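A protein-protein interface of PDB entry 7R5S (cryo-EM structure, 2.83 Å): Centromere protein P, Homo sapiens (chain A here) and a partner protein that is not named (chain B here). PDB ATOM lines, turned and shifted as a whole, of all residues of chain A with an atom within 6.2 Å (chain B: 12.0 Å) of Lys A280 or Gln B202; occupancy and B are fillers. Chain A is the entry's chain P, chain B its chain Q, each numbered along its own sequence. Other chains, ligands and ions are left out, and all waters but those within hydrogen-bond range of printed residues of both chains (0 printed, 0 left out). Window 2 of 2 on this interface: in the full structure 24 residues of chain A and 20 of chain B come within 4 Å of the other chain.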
ATOM      1  N   TYR A 191     -28.468 -36.849 -12.215  1.00  0.00           N
ATOM      2  CA  TYR A 191     -27.514 -37.087 -11.134  1.00  0.00           C
ATOM      3  C   TYR A 191     -28.281 -37.310  -9.836  1.00  0.00           C
ATOM      4  O   TYR A 191     -28.301 -36.438  -8.955  1.00  0.00           O
ATOM      5  CB  TYR A 191     -26.534 -35.924 -10.990  1.00  0.00           C
ATOM      6  CG  TYR A 191     -25.531 -35.814 -12.117  1.00  0.00           C
ATOM      7  CD1 TYR A 191     -24.363 -36.564 -12.108  1.00  0.00           C
ATOM      8  CD2 TYR A 191     -25.749 -34.954 -13.185  1.00  0.00           C
ATOM      9  CE1 TYR A 191     -23.442 -36.465 -13.133  1.00  0.00           C
ATOM     10  CE2 TYR A 191     -24.834 -34.848 -14.215  1.00  0.00           C
ATOM     11  CZ  TYR A 191     -23.682 -35.605 -14.184  1.00  0.00           C
ATOM     12  OH  TYR A 191     -22.768 -35.503 -15.207  1.00  0.00           O
ATOM     13  N   LEU A 269     -20.916 -19.282 -19.386  1.00  0.00           N
ATOM     14  CA  LEU A 269     -21.317 -20.263 -20.386  1.00  0.00           C
ATOM     15  C   LEU A 269     -22.732 -20.798 -20.193  1.00  0.00           C
ATOM     16  O   LEU A 269     -23.099 -21.776 -20.858  1.00  0.00           O
ATOM     17  CB  LEU A 269     -20.325 -21.436 -20.410  1.00  0.00           C
ATOM     18  CG  LEU A 269     -20.270 -22.381 -19.206  1.00  0.00           C
ATOM     19  CD1 LEU A 269     -19.722 -23.734 -19.629  1.00  0.00           C
ATOM     20  CD2 LEU A 269     -19.427 -21.800 -18.078  1.00  0.00           C
ATOM     21  N   LEU A 275     -24.299 -25.303 -13.504  1.00  0.00           N
ATOM     22  CA  LEU A 275     -24.815 -26.234 -12.505  1.00  0.00           C
ATOM     23  C   LEU A 275     -24.168 -27.607 -12.646  1.00  0.00           C
ATOM     24  O   LEU A 275     -23.704 -28.192 -11.660  1.00  0.00           O
ATOM     25  CB  LEU A 275     -26.337 -26.339 -12.620  1.00  0.00           C
ATOM     26  CG  LEU A 275     -27.134 -25.071 -12.305  1.00  0.00           C
ATOM     27  CD1 LEU A 275     -28.628 -25.340 -12.398  1.00  0.00           C
ATOM     28  CD2 LEU A 275     -26.766 -24.530 -10.934  1.00  0.00           C
ATOM     29  N   GLU A 276     -24.125 -28.138 -13.871  1.00  0.00           N
ATOM     30  CA  GLU A 276     -23.521 -29.451 -14.069  1.00  0.00           C
ATOM     31  C   GLU A 276     -22.013 -29.413 -13.847  1.00  0.00           C
ATOM     32  O   GLU A 276     -21.434 -30.405 -13.394  1.00  0.00           O
ATOM     33  CB  GLU A 276     -23.851 -29.992 -15.462  1.00  0.00           C
ATOM     34  CG  GLU A 276     -23.293 -29.184 -16.617  1.00  0.00           C
ATOM     35  CD  GLU A 276     -23.896 -29.585 -17.949  1.00  0.00           C
ATOM     36  OE1 GLU A 276     -23.129 -29.786 -18.914  1.00  0.00           O
ATOM     37  OE2 GLU A 276     -25.137 -29.699 -18.031  1.00  0.00           O
ATOM     38  N   SER A 277     -21.364 -28.279 -14.130  1.00  0.00           N
ATOM     39  CA  SER A 277     -19.945 -28.153 -13.814  1.00  0.00           C
ATOM     40  C   SER A 277     -19.713 -28.203 -12.310  1.00  0.00           C
ATOM     41  O   SER A 277     -18.774 -28.858 -11.843  1.00  0.00           O
ATOM     42  CB  SER A 277     -19.389 -26.855 -14.402  1.00  0.00           C
ATOM     43  OG  SER A 277     -19.628 -25.760 -13.534  1.00  0.00           O
ATOM     44  N   LEU A 278     -20.561 -27.522 -11.536  1.00  0.00           N
ATOM     45  CA  LEU A 278     -20.442 -27.582 -10.083  1.00  0.00           C
ATOM     46  C   LEU A 278     -20.711 -28.991  -9.568  1.00  0.00           C
ATOM     47  O   LEU A 278     -20.040 -29.461  -8.640  1.00  0.00           O
ATOM     48  CB  LEU A 278     -21.396 -26.579  -9.434  1.00  0.00           C
ATOM     49  CG  LEU A 278     -20.921 -25.957  -8.120  1.00  0.00           C
ATOM     50  CD1 LEU A 278     -19.647 -25.157  -8.337  1.00  0.00           C
ATOM     51  CD2 LEU A 278     -22.008 -25.085  -7.513  1.00  0.00           C
ATOM     52  N   ILE A 279     -21.683 -29.684 -10.166  1.00  0.00           N
ATOM     53  CA  ILE A 279     -21.970 -31.060  -9.765  1.00  0.00           C
ATOM     54  C   ILE A 279     -20.772 -31.961 -10.046  1.00  0.00           C
ATOM     55  O   ILE A 279     -20.398 -32.798  -9.216  1.00  0.00           O
ATOM     56  CB  ILE A 279     -23.240 -31.575 -10.469  1.00  0.00           C
ATOM     57  CG1 ILE A 279     -24.466 -30.780 -10.016  1.00  0.00           C
ATOM     58  CG2 ILE A 279     -23.438 -33.060 -10.201  1.00  0.00           C
ATOM     59  CD1 ILE A 279     -25.598 -30.779 -11.020  1.00  0.00           C
ATOM     60  N   LYS A 280     -20.147 -31.798 -11.215  1.00  0.00           N
ATOM     61  CA  LYS A 280     -19.003 -32.633 -11.563  1.00  0.00           C
ATOM     62  C   LYS A 280     -17.795 -32.314 -10.691  1.00  0.00           C
ATOM     63  O   LYS A 280     -17.016 -33.211 -10.351  1.00  0.00           O
ATOM     64  CB  LYS A 280     -18.657 -32.461 -13.043  1.00  0.00           C
ATOM     65  CG  LYS A 280     -19.666 -33.088 -13.990  1.00  0.00           C
ATOM     66  CD  LYS A 280     -19.186 -33.018 -15.431  1.00  0.00           C
ATOM     67  CE  LYS A 280     -20.170 -33.693 -16.372  1.00  0.00           C
ATOM     68  NZ  LYS A 280     -19.697 -33.664 -17.783  1.00  0.00           N
ATOM     69  N   SER A 281     -17.620 -31.043 -10.319  1.00  0.00           N
ATOM     70  CA  SER A 281     -16.496 -30.685  -9.461  1.00  0.00           C
ATOM     71  C   SER A 281     -16.694 -31.212  -8.046  1.00  0.00           C
ATOM     72  O   SER A 281     -15.742 -31.687  -7.416  1.00  0.00           O
ATOM     73  CB  SER A 281     -16.300 -29.169  -9.446  1.00  0.00           C
ATOM     74  OG  SER A 281     -17.531 -28.497  -9.268  1.00  0.00           O
ATOM     75  N   LEU A 282     -17.922 -31.138  -7.526  1.00  0.00           N
ATOM     76  CA  LEU A 282     -18.177 -31.683  -6.197  1.00  0.00           C
ATOM     77  C   LEU A 282     -18.165 -33.206  -6.206  1.00  0.00           C
ATOM     78  O   LEU A 282     -17.927 -33.830  -5.165  1.00  0.00           O
ATOM     79  CB  LEU A 282     -19.507 -31.164  -5.655  1.00  0.00           C
ATOM     80  CG  LEU A 282     -19.709 -31.349  -4.148  1.00  0.00           C
ATOM     81  CD1 LEU A 282     -18.853 -30.362  -3.371  1.00  0.00           C
ATOM     82  CD2 LEU A 282     -21.174 -31.210  -3.768  1.00  0.00           C
ATOM     83  N   CYS A 283     -18.415 -33.822  -7.357  1.00  0.00           N
ATOM     84  CA  CYS A 283     -18.399 -35.276  -7.467  1.00  0.00           C
ATOM     85  C   CYS A 283     -16.975 -35.816  -7.366  1.00  0.00           C
ATOM     86  O   CYS A 283     -16.696 -36.716  -6.575  1.00  0.00           O
ATOM     87  CB  CYS A 283     -19.039 -35.726  -8.781  1.00  0.00           C
ATOM     88  SG  CYS A 283     -18.734 -37.456  -9.206  1.00  0.00           S
ATOM     89  N   GLU B 193      -6.595 -20.525 -24.897  1.00  0.00           N
ATOM     90  CA  GLU B 193      -7.042 -20.573 -23.509  1.00  0.00           C
ATOM     91  C   GLU B 193      -8.529 -20.894 -23.411  1.00  0.00           C
ATOM     92  O   GLU B 193      -8.952 -21.588 -22.477  1.00  0.00           O
ATOM     93  CB  GLU B 193      -6.711 -19.267 -22.781  1.00  0.00           C
ATOM     94  CG  GLU B 193      -7.441 -18.029 -23.263  1.00  0.00           C
ATOM     95  CD  GLU B 193      -6.497 -17.008 -23.863  1.00  0.00           C
ATOM     96  OE1 GLU B 193      -6.787 -15.798 -23.768  1.00  0.00           O
ATOM     97  OE2 GLU B 193      -5.462 -17.414 -24.432  1.00  0.00           O
ATOM     98  N   GLU B 194      -9.345 -20.423 -24.362  1.00  0.00           N
ATOM     99  CA  GLU B 194     -10.751 -20.811 -24.293  1.00  0.00           C
ATOM    100  C   GLU B 194     -10.962 -22.270 -24.677  1.00  0.00           C
ATOM    101  O   GLU B 194     -12.036 -22.815 -24.402  1.00  0.00           O
ATOM    102  CB  GLU B 194     -11.626 -19.905 -25.171  1.00  0.00           C
ATOM    103  CG  GLU B 194     -11.297 -19.882 -26.656  1.00  0.00           C
ATOM    104  CD  GLU B 194     -11.921 -21.039 -27.423  1.00  0.00           C
ATOM    105  OE1 GLU B 194     -12.899 -21.629 -26.920  1.00  0.00           O
ATOM    106  OE2 GLU B 194     -11.437 -21.355 -28.530  1.00  0.00           O
ATOM    107  N   GLU B 195      -9.978 -22.904 -25.316  1.00  0.00           N
ATOM    108  CA  GLU B 195     -10.033 -24.343 -25.543  1.00  0.00           C
ATOM    109  C   GLU B 195      -9.469 -25.128 -24.364  1.00  0.00           C
ATOM    110  O   GLU B 195     -10.000 -26.189 -24.016  1.00  0.00           O
ATOM    111  CB  GLU B 195      -9.276 -24.702 -26.825  1.00  0.00           C
ATOM    112  CG  GLU B 195      -9.653 -26.050 -27.429  1.00  0.00           C
ATOM    113  CD  GLU B 195      -8.951 -27.213 -26.757  1.00  0.00           C
ATOM    114  OE1 GLU B 195      -9.645 -28.076 -26.179  1.00  0.00           O
ATOM    115  OE2 GLU B 195      -7.704 -27.263 -26.802  1.00  0.00           O
ATOM    116  N   ARG B 196      -8.399 -24.626 -23.741  1.00  0.00           N
ATOM    117  CA  ARG B 196      -7.821 -25.298 -22.582  1.00  0.00           C
ATOM    118  C   ARG B 196      -8.746 -25.233 -21.373  1.00  0.00           C
ATOM    119  O   ARG B 196      -8.739 -26.148 -20.540  1.00  0.00           O
ATOM    120  CB  ARG B 196      -6.459 -24.682 -22.253  1.00  0.00           C
ATOM    121  CG  ARG B 196      -5.842 -25.143 -20.939  1.00  0.00           C
ATOM    122  CD  ARG B 196      -4.534 -24.419 -20.662  1.00  0.00           C
ATOM    123  NE  ARG B 196      -4.097 -24.586 -19.278  1.00  0.00           N
ATOM    124  CZ  ARG B 196      -4.434 -23.769 -18.286  1.00  0.00           C
ATOM    125  NH1 ARG B 196      -5.216 -22.724 -18.522  1.00  0.00           N
ATOM    126  NH2 ARG B 196      -3.991 -23.996 -17.056  1.00  0.00           N
ATOM    127  N   VAL B 197      -9.554 -24.173 -21.264  1.00  0.00           N
ATOM    128  CA  VAL B 197     -10.449 -24.032 -20.118  1.00  0.00           C
ATOM    129  C   VAL B 197     -11.443 -25.186 -20.048  1.00  0.00           C
ATOM    130  O   VAL B 197     -11.923 -25.537 -18.963  1.00  0.00           O
ATOM    131  CB  VAL B 197     -11.166 -22.665 -20.166  1.00  0.00           C
ATOM    132  CG1 VAL B 197     -12.225 -22.645 -21.254  1.00  0.00           C
ATOM    133  CG2 VAL B 197     -11.790 -22.345 -18.820  1.00  0.00           C
ATOM    134  N   LYS B 198     -11.760 -25.800 -21.188  1.00  0.00           N
ATOM    135  CA  LYS B 198     -12.714 -26.901 -21.248  1.00  0.00           C
ATOM    136  C   LYS B 198     -12.034 -28.248 -21.474  1.00  0.00           C
ATOM    137  O   LYS B 198     -12.573 -29.104 -22.182  1.00  0.00           O
ATOM    138  CB  LYS B 198     -13.753 -26.636 -22.336  1.00  0.00           C
ATOM    139  CG  LYS B 198     -14.631 -25.426 -22.062  1.00  0.00           C
ATOM    140  CD  LYS B 198     -15.650 -25.215 -23.167  1.00  0.00           C
ATOM    141  CE  LYS B 198     -16.592 -24.070 -22.838  1.00  0.00           C
ATOM    142  NZ  LYS B 198     -17.601 -23.855 -23.913  1.00  0.00           N
ATOM    143  N   GLN B 199     -10.854 -28.451 -20.884  1.00  0.00           N
ATOM    144  CA  GLN B 199     -10.166 -29.731 -21.027  1.00  0.00           C
ATOM    145  C   GLN B 199     -10.846 -30.814 -20.199  1.00  0.00           C
ATOM    146  O   GLN B 199     -11.259 -31.850 -20.732  1.00  0.00           O
ATOM    147  CB  GLN B 199      -8.698 -29.584 -20.627  1.00  0.00           C
ATOM    148  N   MET B 200     -10.969 -30.592 -18.893  1.00  0.00           N
ATOM    149  CA  MET B 200     -11.625 -31.536 -17.997  1.00  0.00           C
ATOM    150  C   MET B 200     -13.115 -31.267 -17.841  1.00  0.00           C
ATOM    151  O   MET B 200     -13.794 -32.015 -17.130  1.00  0.00           O
ATOM    152  CB  MET B 200     -10.953 -31.509 -16.621  1.00  0.00           C
ATOM    153  CG  MET B 200     -11.040 -30.167 -15.915  1.00  0.00           C
ATOM    154  SD  MET B 200     -10.210 -28.846 -16.820  1.00  0.00           S
ATOM    155  CE  MET B 200      -8.519 -29.435 -16.807  1.00  0.00           C
ATOM    156  N   HIS B 201     -13.637 -30.224 -18.481  1.00  0.00           N
ATOM    157  CA  HIS B 201     -15.039 -29.848 -18.378  1.00  0.00           C
ATOM    158  C   HIS B 201     -15.697 -29.936 -19.749  1.00  0.00           C
ATOM    159  O   HIS B 201     -15.073 -29.625 -20.768  1.00  0.00           O
ATOM    160  CB  HIS B 201     -15.182 -28.432 -17.808  1.00  0.00           C
ATOM    161  CG  HIS B 201     -16.561 -27.863 -17.932  1.00  0.00           C
ATOM    162  ND1 HIS B 201     -17.691 -28.560 -17.559  1.00  0.00           N
ATOM    163  CD2 HIS B 201     -16.992 -26.662 -18.382  1.00  0.00           C
ATOM    164  CE1 HIS B 201     -18.758 -27.813 -17.779  1.00  0.00           C
ATOM    165  NE2 HIS B 201     -18.362 -26.657 -18.278  1.00  0.00           N
ATOM    166  N   GLN B 202     -16.957 -30.370 -19.764  1.00  0.00           N
ATOM    167  CA  GLN B 202     -17.713 -30.451 -21.005  1.00  0.00           C
ATOM    168  C   GLN B 202     -17.890 -29.059 -21.609  1.00  0.00           C
ATOM    169  O   GLN B 202     -17.857 -28.041 -20.913  1.00  0.00           O
ATOM    170  CB  GLN B 202     -19.075 -31.102 -20.754  1.00  0.00           C
ATOM    171  CG  GLN B 202     -19.790 -31.579 -22.011  1.00  0.00           C
ATOM    172  CD  GLN B 202     -21.238 -31.945 -21.756  1.00  0.00           C
ATOM    173  OE1 GLN B 202     -21.950 -32.375 -22.663  1.00  0.00           O
ATOM    174  NE2 GLN B 202     -21.682 -31.775 -20.515  1.00  0.00           N
ATOM    175  N   ILE B 203     -18.068 -29.023 -22.932  1.00  0.00           N
ATOM    176  CA  ILE B 203     -18.201 -27.747 -23.633  1.00  0.00           C
ATOM    177  C   ILE B 203     -19.439 -27.002 -23.147  1.00  0.00           C
ATOM    178  O   ILE B 203     -19.349 -25.903 -22.588  1.00  0.00           O
ATOM    179  CB  ILE B 203     -18.242 -27.969 -25.157  1.00  0.00           C
ATOM    180  CG1 ILE B 203     -17.050 -28.812 -25.620  1.00  0.00           C
ATOM    181  CG2 ILE B 203     -18.258 -26.636 -25.887  1.00  0.00           C
ATOM    182  CD1 ILE B 203     -15.713 -28.348 -25.084  1.00  0.00           C
ATOM    183  N   ASN B 204     -20.611 -27.595 -23.353  1.00  0.00           N
ATOM    184  CA  ASN B 204     -21.870 -27.048 -22.856  1.00  0.00           C
ATOM    185  C   ASN B 204     -22.813 -28.180 -22.456  1.00  0.00           C
ATOM    186  O   ASN B 204     -23.355 -28.187 -21.352  1.00  0.00           O
ATOM    187  CB  ASN B 204     -22.547 -26.153 -23.904  1.00  0.00           C
ATOM    188  CG  ASN B 204     -21.630 -25.066 -24.434  1.00  0.00           C
ATOM    189  OD1 ASN B 204     -21.220 -24.171 -23.696  1.00  0.00           O
ATOM    190  ND2 ASN B 204     -21.307 -25.138 -25.720  1.00  0.00           N
ATOM    191  N   LEU B 209     -32.508 -28.140 -23.980  1.00  0.00           N
ATOM    192  CA  LEU B 209     -32.821 -27.104 -23.003  1.00  0.00           C
ATOM    193  C   LEU B 209     -32.369 -25.734 -23.500  1.00  0.00           C
ATOM    194  O   LEU B 209     -31.232 -25.324 -23.267  1.00  0.00           O
ATOM    195  CB  LEU B 209     -32.170 -27.416 -21.653  1.00  0.00           C
ATOM    196  CG  LEU B 209     -32.715 -28.608 -20.861  1.00  0.00           C
ATOM    197  CD1 LEU B 209     -32.050 -29.909 -21.288  1.00  0.00           C
ATOM    198  CD2 LEU B 209     -32.545 -28.379 -19.366  1.00  0.00           C
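O of Asn B204 lies close to OE1 of Glu A276 (2.9 Å). NE2 of Gln B202 is in hydrogen-bond range of OE1 of Glu A276.
OG of Ser A281 sits at hydrogen-bond distance from O of Ser A277 (2.9 Å). The backbone carbonyl oxygen of Ile B203 sits at hydrogen-bond distance from the side-chain amino group of Lys B198.
His B201 touches Leu A269. CD1 of Leu A269 touches O of Ile B203, 3.7 Å away. CE1 of His B201 touches CB of Ser A277 (3.6 Å). NZ of Lys A280 touches NE2 of Gln B202, 3.9 Å away.
Printed residues of chain B within 4 Å of Leu A269: His B201 (3.5 Å) and Ile B203 (3.7 Å). Glu A276 touches just these residues of chain B: Gln B202 and Asn B204. Of chain B, only His B201 comes within 4 Å of Ser A277. No residue of chain B comes within 4 Å of Leu A278. Ile A279 touches none of the printed residues of chain B. Of chain B, only Gln B202 comes within 4 Å of Lys A280. No residue of chain B comes within 4 Å of Ser A281. No residue of chain B comes within 4 Å of Leu A282. No residue of chain B comes within 4 Å of Cys A283. Of the printed residues of chain A, His B201 touches Leu A269 and Ser A277. Gln B202 touches just these residues of chain A: Glu A276 and Lys A280. Of the printed residues of chain A, Ile B203 touches Leu A269 (3.7 Å). The nearest residue of chain B that does not touch Lys A280 is His B201 (5.2 Å). The nearest printed residue of chain A that does not touch Asn B204 is Leu A269 (4.2 Å).
Hydrophobic or aromatic side chains of chain B within 4 Å of the printed part of chain A: His B201. Of the 11 printed residues of chain A, 4 touch a printed residue of chain B. Among the printed residues, no Asp or Glu carboxylate lies within 4 Å of a Lys or Arg side-chain nitrogen of the other chain.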
